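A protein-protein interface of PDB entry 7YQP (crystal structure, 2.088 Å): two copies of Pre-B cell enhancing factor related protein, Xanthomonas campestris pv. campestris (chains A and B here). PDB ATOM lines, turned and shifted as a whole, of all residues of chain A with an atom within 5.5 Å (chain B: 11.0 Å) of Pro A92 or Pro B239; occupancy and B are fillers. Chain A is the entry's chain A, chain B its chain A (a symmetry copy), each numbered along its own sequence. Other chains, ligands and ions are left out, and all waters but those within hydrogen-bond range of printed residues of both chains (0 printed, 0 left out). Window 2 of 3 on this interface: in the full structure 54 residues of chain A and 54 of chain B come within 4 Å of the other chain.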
ATOM      1  N   TYR A  28      13.953  24.403   1.221  1.00  0.00           N
ATOM      2  CA  TYR A  28      14.477  23.047   1.121  1.00  0.00           C
ATOM      3  C   TYR A  28      13.680  22.189   0.148  1.00  0.00           C
ATOM      4  O   TYR A  28      14.219  21.207  -0.373  1.00  0.00           O
ATOM      5  CB  TYR A  28      14.534  22.388   2.506  1.00  0.00           C
ATOM      6  CG  TYR A  28      13.201  22.144   3.186  1.00  0.00           C
ATOM      7  CD1 TYR A  28      12.412  21.050   2.853  1.00  0.00           C
ATOM      8  CD2 TYR A  28      12.747  22.992   4.186  1.00  0.00           C
ATOM      9  CE1 TYR A  28      11.200  20.823   3.483  1.00  0.00           C
ATOM     10  CE2 TYR A  28      11.539  22.773   4.823  1.00  0.00           C
ATOM     11  CZ  TYR A  28      10.770  21.688   4.468  1.00  0.00           C
ATOM     12  OH  TYR A  28       9.568  21.467   5.100  1.00  0.00           O
ATOM     13  N   ALA A  30      12.750  23.063  -2.815  1.00  0.00           N
ATOM     14  CA  ALA A  30      13.325  23.213  -4.147  1.00  0.00           C
ATOM     15  C   ALA A  30      14.419  22.181  -4.385  1.00  0.00           C
ATOM     16  O   ALA A  30      14.571  21.668  -5.500  1.00  0.00           O
ATOM     17  CB  ALA A  30      13.870  24.628  -4.329  1.00  0.00           C
ATOM     18  N   SER A  31      15.189  21.863  -3.347  1.00  0.00           N
ATOM     19  CA  SER A  31      16.249  20.865  -3.409  1.00  0.00           C
ATOM     20  C   SER A  31      15.738  19.441  -3.239  1.00  0.00           C
ATOM     21  O   SER A  31      16.551  18.511  -3.209  1.00  0.00           O
ATOM     22  CB  SER A  31      17.289  21.154  -2.325  1.00  0.00           C
ATOM     23  OG  SER A  31      16.730  20.969  -1.033  1.00  0.00           O
ATOM     24  N   TRP A  33      13.884  17.208  -5.004  1.00  0.00           N
ATOM     25  CA  TRP A  33      13.811  16.165  -6.022  1.00  0.00           C
ATOM     26  C   TRP A  33      15.048  15.273  -6.028  1.00  0.00           C
ATOM     27  O   TRP A  33      14.967  14.123  -6.473  1.00  0.00           O
ATOM     28  CB  TRP A  33      13.585  16.781  -7.408  1.00  0.00           C
ATOM     29  CG  TRP A  33      14.837  17.067  -8.192  1.00  0.00           C
ATOM     30  CD1 TRP A  33      15.362  16.312  -9.201  1.00  0.00           C
ATOM     31  CD2 TRP A  33      15.703  18.203  -8.050  1.00  0.00           C
ATOM     32  NE1 TRP A  33      16.508  16.898  -9.687  1.00  0.00           N
ATOM     33  CE2 TRP A  33      16.739  18.059  -8.997  1.00  0.00           C
ATOM     34  CE3 TRP A  33      15.708  19.320  -7.212  1.00  0.00           C
ATOM     35  CZ2 TRP A  33      17.768  18.993  -9.127  1.00  0.00           C
ATOM     36  CZ3 TRP A  33      16.730  20.246  -7.342  1.00  0.00           C
ATOM     37  CH2 TRP A  33      17.745  20.077  -8.293  1.00  0.00           C
ATOM     38  N   LEU A  34      16.182  15.765  -5.528  1.00  0.00           N
ATOM     39  CA  LEU A  34      17.393  14.956  -5.462  1.00  0.00           C
ATOM     40  C   LEU A  34      17.349  13.913  -4.354  1.00  0.00           C
ATOM     41  O   LEU A  34      18.183  13.002  -4.352  1.00  0.00           O
ATOM     42  CB  LEU A  34      18.612  15.855  -5.265  1.00  0.00           C
ATOM     43  CG  LEU A  34      18.922  16.799  -6.425  1.00  0.00           C
ATOM     44  CD1 LEU A  34      19.511  18.102  -5.909  1.00  0.00           C
ATOM     45  CD2 LEU A  34      19.860  16.130  -7.420  1.00  0.00           C
ATOM     46  N   LEU A  86      17.439  31.511  -6.272  1.00  0.00           N
ATOM     47  CA  LEU A  86      17.750  30.397  -5.380  1.00  0.00           C
ATOM     48  C   LEU A  86      19.236  30.062  -5.354  1.00  0.00           C
ATOM     49  O   LEU A  86      19.739  29.587  -4.327  1.00  0.00           O
ATOM     50  CB  LEU A  86      16.933  29.162  -5.768  1.00  0.00           C
ATOM     51  CG  LEU A  86      15.453  29.298  -5.412  1.00  0.00           C
ATOM     52  CD1 LEU A  86      14.534  28.710  -6.491  1.00  0.00           C
ATOM     53  CD2 LEU A  86      15.188  28.688  -4.039  1.00  0.00           C
ATOM     54  N   GLY A  90      21.072  29.889  -1.844  1.00  0.00           N
ATOM     55  CA  GLY A  90      21.791  28.752  -1.302  1.00  0.00           C
ATOM     56  C   GLY A  90      21.128  27.411  -1.540  1.00  0.00           C
ATOM     57  O   GLY A  90      21.501  26.418  -0.909  1.00  0.00           O
ATOM     58  N   GLU A  91      20.151  27.359  -2.447  1.00  0.00           N
ATOM     59  CA  GLU A  91      19.430  26.122  -2.696  1.00  0.00           C
ATOM     60  C   GLU A  91      19.646  25.636  -4.124  1.00  0.00           C
ATOM     61  O   GLU A  91      19.699  26.446  -5.056  1.00  0.00           O
ATOM     62  CB  GLU A  91      17.921  26.298  -2.453  1.00  0.00           C
ATOM     63  CG  GLU A  91      17.537  26.451  -0.993  1.00  0.00           C
ATOM     64  CD  GLU A  91      17.593  25.141  -0.226  1.00  0.00           C
ATOM     65  OE1 GLU A  91      17.646  24.070  -0.868  1.00  0.00           O
ATOM     66  OE2 GLU A  91      17.576  25.185   1.022  1.00  0.00           O
ATOM     67  N   PRO A  92      19.774  24.326  -4.325  1.00  0.00           N
ATOM     68  CA  PRO A  92      19.761  23.789  -5.688  1.00  0.00           C
ATOM     69  C   PRO A  92      18.394  23.971  -6.321  1.00  0.00           C
ATOM     70  O   PRO A  92      17.370  24.052  -5.638  1.00  0.00           O
ATOM     71  CB  PRO A  92      20.092  22.302  -5.497  1.00  0.00           C
ATOM     72  CG  PRO A  92      20.573  22.169  -4.085  1.00  0.00           C
ATOM     73  CD  PRO A  92      19.942  23.275  -3.311  1.00  0.00           C
ATOM     74  N   PHE A  93      18.381  24.030  -7.648  1.00  0.00           N
ATOM     75  CA  PHE A  93      17.145  24.250  -8.381  1.00  0.00           C
ATOM     76  C   PHE A  93      17.136  23.378  -9.625  1.00  0.00           C
ATOM     77  O   PHE A  93      18.086  23.408 -10.412  1.00  0.00           O
ATOM     78  CB  PHE A  93      16.991  25.725  -8.757  1.00  0.00           C
ATOM     79  CG  PHE A  93      15.745  26.025  -9.527  1.00  0.00           C
ATOM     80  CD1 PHE A  93      14.501  25.893  -8.935  1.00  0.00           C
ATOM     81  CD2 PHE A  93      15.815  26.438 -10.848  1.00  0.00           C
ATOM     82  CE1 PHE A  93      13.352  26.168  -9.644  1.00  0.00           C
ATOM     83  CE2 PHE A  93      14.668  26.715 -11.562  1.00  0.00           C
ATOM     84  CZ  PHE A  93      13.436  26.581 -10.960  1.00  0.00           C
ATOM     85  N   ASN A  94      16.060  22.606  -9.798  1.00  0.00           N
ATOM     86  CA  ASN A  94      15.929  21.685 -10.927  1.00  0.00           C
ATOM     87  C   ASN A  94      15.480  22.460 -12.166  1.00  0.00           C
ATOM     88  O   ASN A  94      14.327  22.402 -12.604  1.00  0.00           O
ATOM     89  CB  ASN A  94      14.956  20.563 -10.589  1.00  0.00           C
ATOM     90  CG  ASN A  94      14.962  19.450 -11.624  1.00  0.00           C
ATOM     91  OD1 ASN A  94      15.704  19.498 -12.608  1.00  0.00           O
ATOM     92  ND2 ASN A  94      14.130  18.439 -11.404  1.00  0.00           N
ATOM     93  N   HIS B 189      16.230  30.410  12.494  1.00  0.00           N
ATOM     94  CA  HIS B 189      15.847  30.157  11.113  1.00  0.00           C
ATOM     95  C   HIS B 189      14.330  30.084  11.008  1.00  0.00           C
ATOM     96  O   HIS B 189      13.668  29.484  11.862  1.00  0.00           O
ATOM     97  CB  HIS B 189      16.478  28.854  10.612  1.00  0.00           C
ATOM     98  CG  HIS B 189      16.609  28.775   9.126  1.00  0.00           C
ATOM     99  ND1 HIS B 189      17.798  29.013   8.471  1.00  0.00           N
ATOM    100  CD2 HIS B 189      15.703  28.481   8.164  1.00  0.00           C
ATOM    101  CE1 HIS B 189      17.619  28.871   7.170  1.00  0.00           C
ATOM    102  NE2 HIS B 189      16.356  28.548   6.957  1.00  0.00           N
ATOM    103  N   PHE B 191      11.085  28.624   9.500  1.00  0.00           N
ATOM    104  CA  PHE B 191      10.478  27.491   8.810  1.00  0.00           C
ATOM    105  C   PHE B 191       8.957  27.616   8.794  1.00  0.00           C
ATOM    106  O   PHE B 191       8.245  26.609   8.845  1.00  0.00           O
ATOM    107  CB  PHE B 191      10.879  26.167   9.461  1.00  0.00           C
ATOM    108  CG  PHE B 191      12.351  25.877   9.412  1.00  0.00           C
ATOM    109  CD1 PHE B 191      12.999  25.706   8.199  1.00  0.00           C
ATOM    110  CD2 PHE B 191      13.085  25.756  10.583  1.00  0.00           C
ATOM    111  CE1 PHE B 191      14.353  25.428   8.155  1.00  0.00           C
ATOM    112  CE2 PHE B 191      14.444  25.480  10.544  1.00  0.00           C
ATOM    113  CZ  PHE B 191      15.076  25.317   9.329  1.00  0.00           C
ATOM    114  N   THR B 216      16.424  31.923   6.502  1.00  0.00           N
ATOM    115  CA  THR B 216      14.998  31.755   6.267  1.00  0.00           C
ATOM    116  C   THR B 216      14.774  30.698   5.199  1.00  0.00           C
ATOM    117  O   THR B 216      15.552  30.586   4.246  1.00  0.00           O
ATOM    118  CB  THR B 216      14.337  33.074   5.846  1.00  0.00           C
ATOM    119  OG1 THR B 216      12.927  32.875   5.699  1.00  0.00           O
ATOM    120  CG2 THR B 216      14.919  33.589   4.529  1.00  0.00           C
ATOM    121  N   ASP B 217      13.720  29.907   5.386  1.00  0.00           N
ATOM    122  CA  ASP B 217      13.216  29.004   4.363  1.00  0.00           C
ATOM    123  C   ASP B 217      11.952  29.539   3.712  1.00  0.00           C
ATOM    124  O   ASP B 217      11.339  28.841   2.895  1.00  0.00           O
ATOM    125  CB  ASP B 217      12.953  27.621   4.954  1.00  0.00           C
ATOM    126  CG  ASP B 217      14.151  26.711   4.842  1.00  0.00           C
ATOM    127  OD1 ASP B 217      15.246  27.210   4.515  1.00  0.00           O
ATOM    128  OD2 ASP B 217      14.002  25.499   5.085  1.00  0.00           O
ATOM    129  N   LEU B 219      10.762  31.539   1.146  1.00  0.00           N
ATOM    130  CA  LEU B 219      11.091  32.228  -0.097  1.00  0.00           C
ATOM    131  C   LEU B 219      10.213  33.451  -0.301  1.00  0.00           C
ATOM    132  O   LEU B 219      10.663  34.452  -0.872  1.00  0.00           O
ATOM    133  CB  LEU B 219      10.942  31.264  -1.278  1.00  0.00           C
ATOM    134  CG  LEU B 219      12.010  30.171  -1.395  1.00  0.00           C
ATOM    135  CD1 LEU B 219      11.739  29.267  -2.584  1.00  0.00           C
ATOM    136  CD2 LEU B 219      13.400  30.767  -1.491  1.00  0.00           C
ATOM    137  N   TYR B 236      19.354  33.709   3.509  1.00  0.00           N
ATOM    138  CA  TYR B 236      19.984  32.524   2.952  1.00  0.00           C
ATOM    139  C   TYR B 236      19.479  31.280   3.668  1.00  0.00           C
ATOM    140  O   TYR B 236      18.900  31.350   4.757  1.00  0.00           O
ATOM    141  CB  TYR B 236      21.516  32.606   3.057  1.00  0.00           C
ATOM    142  CG  TYR B 236      22.085  33.898   2.507  1.00  0.00           C
ATOM    143  CD1 TYR B 236      22.060  34.166   1.144  1.00  0.00           C
ATOM    144  CD2 TYR B 236      22.636  34.854   3.352  1.00  0.00           C
ATOM    145  CE1 TYR B 236      22.572  35.349   0.634  1.00  0.00           C
ATOM    146  CE2 TYR B 236      23.151  36.040   2.853  1.00  0.00           C
ATOM    147  CZ  TYR B 236      23.117  36.282   1.494  1.00  0.00           C
ATOM    148  OH  TYR B 236      23.623  37.461   0.991  1.00  0.00           O
ATOM    149  N   SER B 237      19.704  30.134   3.033  1.00  0.00           N
ATOM    150  CA  SER B 237      19.428  28.846   3.650  1.00  0.00           C
ATOM    151  C   SER B 237      20.351  27.812   3.022  1.00  0.00           C
ATOM    152  O   SER B 237      21.177  28.125   2.157  1.00  0.00           O
ATOM    153  CB  SER B 237      17.956  28.448   3.496  1.00  0.00           C
ATOM    154  OG  SER B 237      17.710  27.185   4.097  1.00  0.00           O
ATOM    155  N   ILE B 238      20.207  26.568   3.468  1.00  0.00           N
ATOM    156  CA  ILE B 238      21.068  25.478   3.018  1.00  0.00           C
ATOM    157  C   ILE B 238      20.189  24.297   2.622  1.00  0.00           C
ATOM    158  O   ILE B 238      19.069  24.160   3.139  1.00  0.00           O
ATOM    159  CB  ILE B 238      22.075  25.088   4.111  1.00  0.00           C
ATOM    160  CG1 ILE B 238      21.350  24.786   5.422  1.00  0.00           C
ATOM    161  CG2 ILE B 238      23.104  26.193   4.318  1.00  0.00           C
ATOM    162  CD1 ILE B 238      22.281  24.449   6.571  1.00  0.00           C
ATOM    163  N   PRO B 239      20.638  23.427   1.718  1.00  0.00           N
ATOM    164  CA  PRO B 239      19.829  22.257   1.367  1.00  0.00           C
ATOM    165  C   PRO B 239      19.726  21.292   2.536  1.00  0.00           C
ATOM    166  O   PRO B 239      20.655  21.142   3.332  1.00  0.00           O
ATOM    167  CB  PRO B 239      20.594  21.632   0.196  1.00  0.00           C
ATOM    168  CG  PRO B 239      22.008  22.078   0.400  1.00  0.00           C
ATOM    169  CD  PRO B 239      21.909  23.465   0.972  1.00  0.00           C
ATOM    170  N   ALA B 240      18.572  20.640   2.635  1.00  0.00           N
ATOM    171  CA  ALA B 240      18.316  19.707   3.724  1.00  0.00           C
ATOM    172  C   ALA B 240      17.714  18.406   3.202  1.00  0.00           C
ATOM    173  O   ALA B 240      17.886  17.345   3.803  1.00  0.00           O
ATOM    174  CB  ALA B 240      17.398  20.340   4.758  1.00  0.00           C
ATOM    175  N   ALA B 270      30.355  24.980   1.798  1.00  0.00           N
ATOM    176  CA  ALA B 270      29.079  24.287   1.671  1.00  0.00           C
ATOM    177  C   ALA B 270      28.677  23.677   3.005  1.00  0.00           C
ATOM    178  O   ALA B 270      29.482  23.020   3.670  1.00  0.00           O
ATOM    179  CB  ALA B 270      29.155  23.213   0.590  1.00  0.00           C
ATOM    180  N   ILE B 271      27.428  23.911   3.395  1.00  0.00           N
ATOM    181  CA  ILE B 271      26.909  23.497   4.693  1.00  0.00           C
ATOM    182  C   ILE B 271      25.605  22.743   4.457  1.00  0.00           C
ATOM    183  O   ILE B 271      24.654  23.306   3.903  1.00  0.00           O
ATOM    184  CB  ILE B 271      26.690  24.693   5.642  1.00  0.00           C
ATOM    185  CG1 ILE B 271      27.958  25.547   5.805  1.00  0.00           C
ATOM    186  CG2 ILE B 271      26.205  24.222   6.994  1.00  0.00           C
ATOM    187  CD1 ILE B 271      28.151  26.648   4.761  1.00  0.00           C
ATOM    188  N   VAL B 272      25.556  21.476   4.871  1.00  0.00           N
ATOM    189  CA  VAL B 272      24.422  20.597   4.601  1.00  0.00           C
ATOM    190  C   VAL B 272      23.778  20.193   5.921  1.00  0.00           C
ATOM    191  O   VAL B 272      24.475  19.847   6.883  1.00  0.00           O
ATOM    192  CB  VAL B 272      24.850  19.356   3.798  1.00  0.00           C
ATOM    193  CG1 VAL B 272      24.988  19.706   2.323  1.00  0.00           C
ATOM    194  CG2 VAL B 272      26.158  18.801   4.338  1.00  0.00           C
ATOM    195  N   ALA B 273      22.451  20.243   5.967  1.00  0.00           N
ATOM    196  CA  ALA B 273      21.691  19.824   7.136  1.00  0.00           C
ATOM    197  C   ALA B 273      21.084  18.453   6.873  1.00  0.00           C
ATOM    198  O   ALA B 273      20.436  18.245   5.842  1.00  0.00           O
ATOM    199  CB  ALA B 273      20.591  20.832   7.474  1.00  0.00           C
ATOM    200  N   VAL B 274      21.310  17.519   7.793  1.00  0.00           N
ATOM    201  CA  VAL B 274      20.745  16.179   7.708  1.00  0.00           C
ATOM    202  C   VAL B 274      19.764  16.003   8.860  1.00  0.00           C
ATOM    203  O   VAL B 274      20.061  16.371  10.003  1.00  0.00           O
ATOM    204  CB  VAL B 274      21.845  15.096   7.705  1.00  0.00           C
ATOM    205  CG1 VAL B 274      22.931  15.465   6.705  1.00  0.00           C
ATOM    206  CG2 VAL B 274      22.458  14.902   9.085  1.00  0.00           C
ATOM    207  N   VAL B 275      18.578  15.492   8.548  1.00  0.00           N
ATOM    208  CA  VAL B 275      17.522  15.343   9.545  1.00  0.00           C
ATOM    209  C   VAL B 275      17.718  14.014  10.261  1.00  0.00           C
ATOM    210  O   VAL B 275      17.757  12.956   9.624  1.00  0.00           O
ATOM    211  CB  VAL B 275      16.134  15.423   8.895  1.00  0.00           C
ATOM    212  CG1 VAL B 275      15.048  15.189   9.934  1.00  0.00           C
ATOM    213  CG2 VAL B 275      15.949  16.766   8.210  1.00  0.00           C
ATOM    214  N   VAL B 304      28.518  20.014   9.380  1.00  0.00           N
ATOM    215  CA  VAL B 304      27.215  19.378   9.204  1.00  0.00           C
ATOM    216  C   VAL B 304      26.252  19.753  10.320  1.00  0.00           C
ATOM    217  O   VAL B 304      26.569  19.642  11.505  1.00  0.00           O
ATOM    218  CB  VAL B 304      27.352  17.849   9.111  1.00  0.00           C
ATOM    219  CG1 VAL B 304      26.017  17.171   9.415  1.00  0.00           C
ATOM    220  CG2 VAL B 304      27.824  17.464   7.727  1.00  0.00           C
ATOM    221  N   VAL B 305      25.070  20.200   9.928  1.00  0.00           N
ATOM    222  CA  VAL B 305      24.013  20.549  10.866  1.00  0.00           C
ATOM    223  C   VAL B 305      23.055  19.374  10.962  1.00  0.00           C
ATOM    224  O   VAL B 305      22.760  18.714   9.957  1.00  0.00           O
ATOM    225  CB  VAL B 305      23.289  21.835  10.427  1.00  0.00           C
ATOM    226  CG1 VAL B 305      22.583  22.467  11.605  1.00  0.00           C
ATOM    227  CG2 VAL B 305      24.278  22.812   9.812  1.00  0.00           C
ATOM    228  N   ILE B 306      22.578  19.099  12.172  1.00  0.00           N
ATOM    229  CA  ILE B 306      21.647  18.006  12.423  1.00  0.00           C
ATOM    230  C   ILE B 306      20.333  18.606  12.900  1.00  0.00           C
ATOM    231  O   ILE B 306      20.297  19.306  13.920  1.00  0.00           O
ATOM    232  CB  ILE B 306      22.199  17.004  13.448  1.00  0.00           C
ATOM    233  CG1 ILE B 306      23.653  16.660  13.118  1.00  0.00           C
ATOM    234  CG2 ILE B 306      21.340  15.751  13.477  1.00  0.00           C
ATOM    235  CD1 ILE B 306      24.134  15.353  13.719  1.00  0.00           C
ATOM    236  N   ARG B 307      19.257  18.334  12.157  1.00  0.00           N
ATOM    237  CA  ARG B 307      17.915  18.800  12.472  1.00  0.00           C
ATOM    238  C   ARG B 307      17.114  17.641  13.059  1.00  0.00           C
ATOM    239  O   ARG B 307      16.658  16.767  12.307  1.00  0.00           O
ATOM    240  CB  ARG B 307      17.232  19.346  11.213  1.00  0.00           C
ATOM    241  CG  ARG B 307      15.990  20.184  11.488  1.00  0.00           C
ATOM    242  CD  ARG B 307      14.773  19.709  10.693  1.00  0.00           C
ATOM    243  NE  ARG B 307      14.873  20.009   9.264  1.00  0.00           N
ATOM    244  CZ  ARG B 307      13.866  19.900   8.400  1.00  0.00           C
ATOM    245  NH1 ARG B 307      12.671  19.496   8.813  1.00  0.00           N
ATOM    246  NH2 ARG B 307      14.054  20.193   7.120  1.00  0.00           N
ATOM    247  N   ILE B 346      20.710  22.084  14.940  1.00  0.00           N
ATOM    248  CA  ILE B 346      19.618  23.047  14.837  1.00  0.00           C
ATOM    249  C   ILE B 346      18.365  22.411  15.417  1.00  0.00           C
ATOM    250  O   ILE B 346      17.895  21.380  14.922  1.00  0.00           O
ATOM    251  CB  ILE B 346      19.377  23.522  13.393  1.00  0.00           C
ATOM    252  CG1 ILE B 346      18.130  24.408  13.344  1.00  0.00           C
ATOM    253  CG2 ILE B 346      19.227  22.348  12.433  1.00  0.00           C
ATOM    254  CD1 ILE B 346      18.192  25.500  12.304  1.00  0.00           C
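Among the printed residues, pairs that only touch across the chains: Tyr A28 with Asp B217 (2.9 Å), Leu A86 with Leu B219 (3.7 Å), Gly A90 with Ser B237 (3.5 Å), Gly A90 with Pro B239 (3.5 Å), Glu A91 with Ser B237 (3.7 Å), Glu A91 with Pro B239 (3.6 Å) and Pro A92 with Pro B239 (3.9 Å).
The backbone carbonyl oxygen (O) of Tyr A28 sits at hydrogen-bond distance from the side-chain hydroxyl (OG) of Ser A31 (2.6 Å).
OG of Ser A31 sits at hydrogen-bond distance from OE1 of Glu A91, 3.2 Å away.
O of Leu A86 is in hydrogen-bond range of N of Glu A91 (2.9 Å).
A ring nitrogen (NE2) of His B189 sits at hydrogen-bond distance from the side-chain hydroxyl of Ser B237 (3.4 Å).
The side-chain carboxylate (OD1) of Asp B217 sits at hydrogen-bond distance from the side-chain hydroxyl (OG) of Ser B237, 2.5 Å away.
N of Ala B273 is in hydrogen-bond range of O of Pro B239, 3.3 Å away.
No position is printed for both chains.
Of the 8 pairs that touch across the chains among the printed residues, none has its exchanged pair printed and touching as well.
Ser A31 touches none of the printed residues of chain B.
Of the printed residues of chain B, Leu A86 touches Leu B219 (3.7 Å).
Gly A90 touches just these residues of chain B: Ser B237 (3.5 Å) and Pro B239 (3.5 Å).
Glu A91 touches three residues of chain B.
Of chain B, only Pro B239 comes within 4 Å of Pro A92.
Of the printed residues of chain A, Ser B237 touches Gly A90 (3.5 Å) and Glu A91 (3.7 Å).
Printed residues of chain A within 4 Å of Pro B239: Gly A90 (3.5 Å), Glu A91 (3.6 Å) and Pro A92 (3.9 Å).
The nearest residue of chain B that does not touch Pro A92 is Ile B238 (6.0 Å).
The nearest printed residue of chain A that does not touch Leu B219 is Ala A30 (5.4 Å).
The side-chain carboxylate (OE2) of Glu A91 lies close to the backbone carbonyl oxygen (O) of Ile B238, at 2.8 Å.
Of the 11 printed residues of chain A, 5 touch a printed residue of chain B.
Printed residues of chain A that touch a printed residue of chain B: Tyr A28, Leu A86, Gly A90, Glu A91 and Pro A92.
Hydrophobic or aromatic side chains of chain A that line the printed part of chain B: Tyr A28, Leu A86 and Pro A92.
Among the printed residues, 8 pairs touch across the chains.
Among the printed residues, no Asp or Glu carboxylate lies within 4 Å of a Lys or Arg side-chain nitrogen of the other chain.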
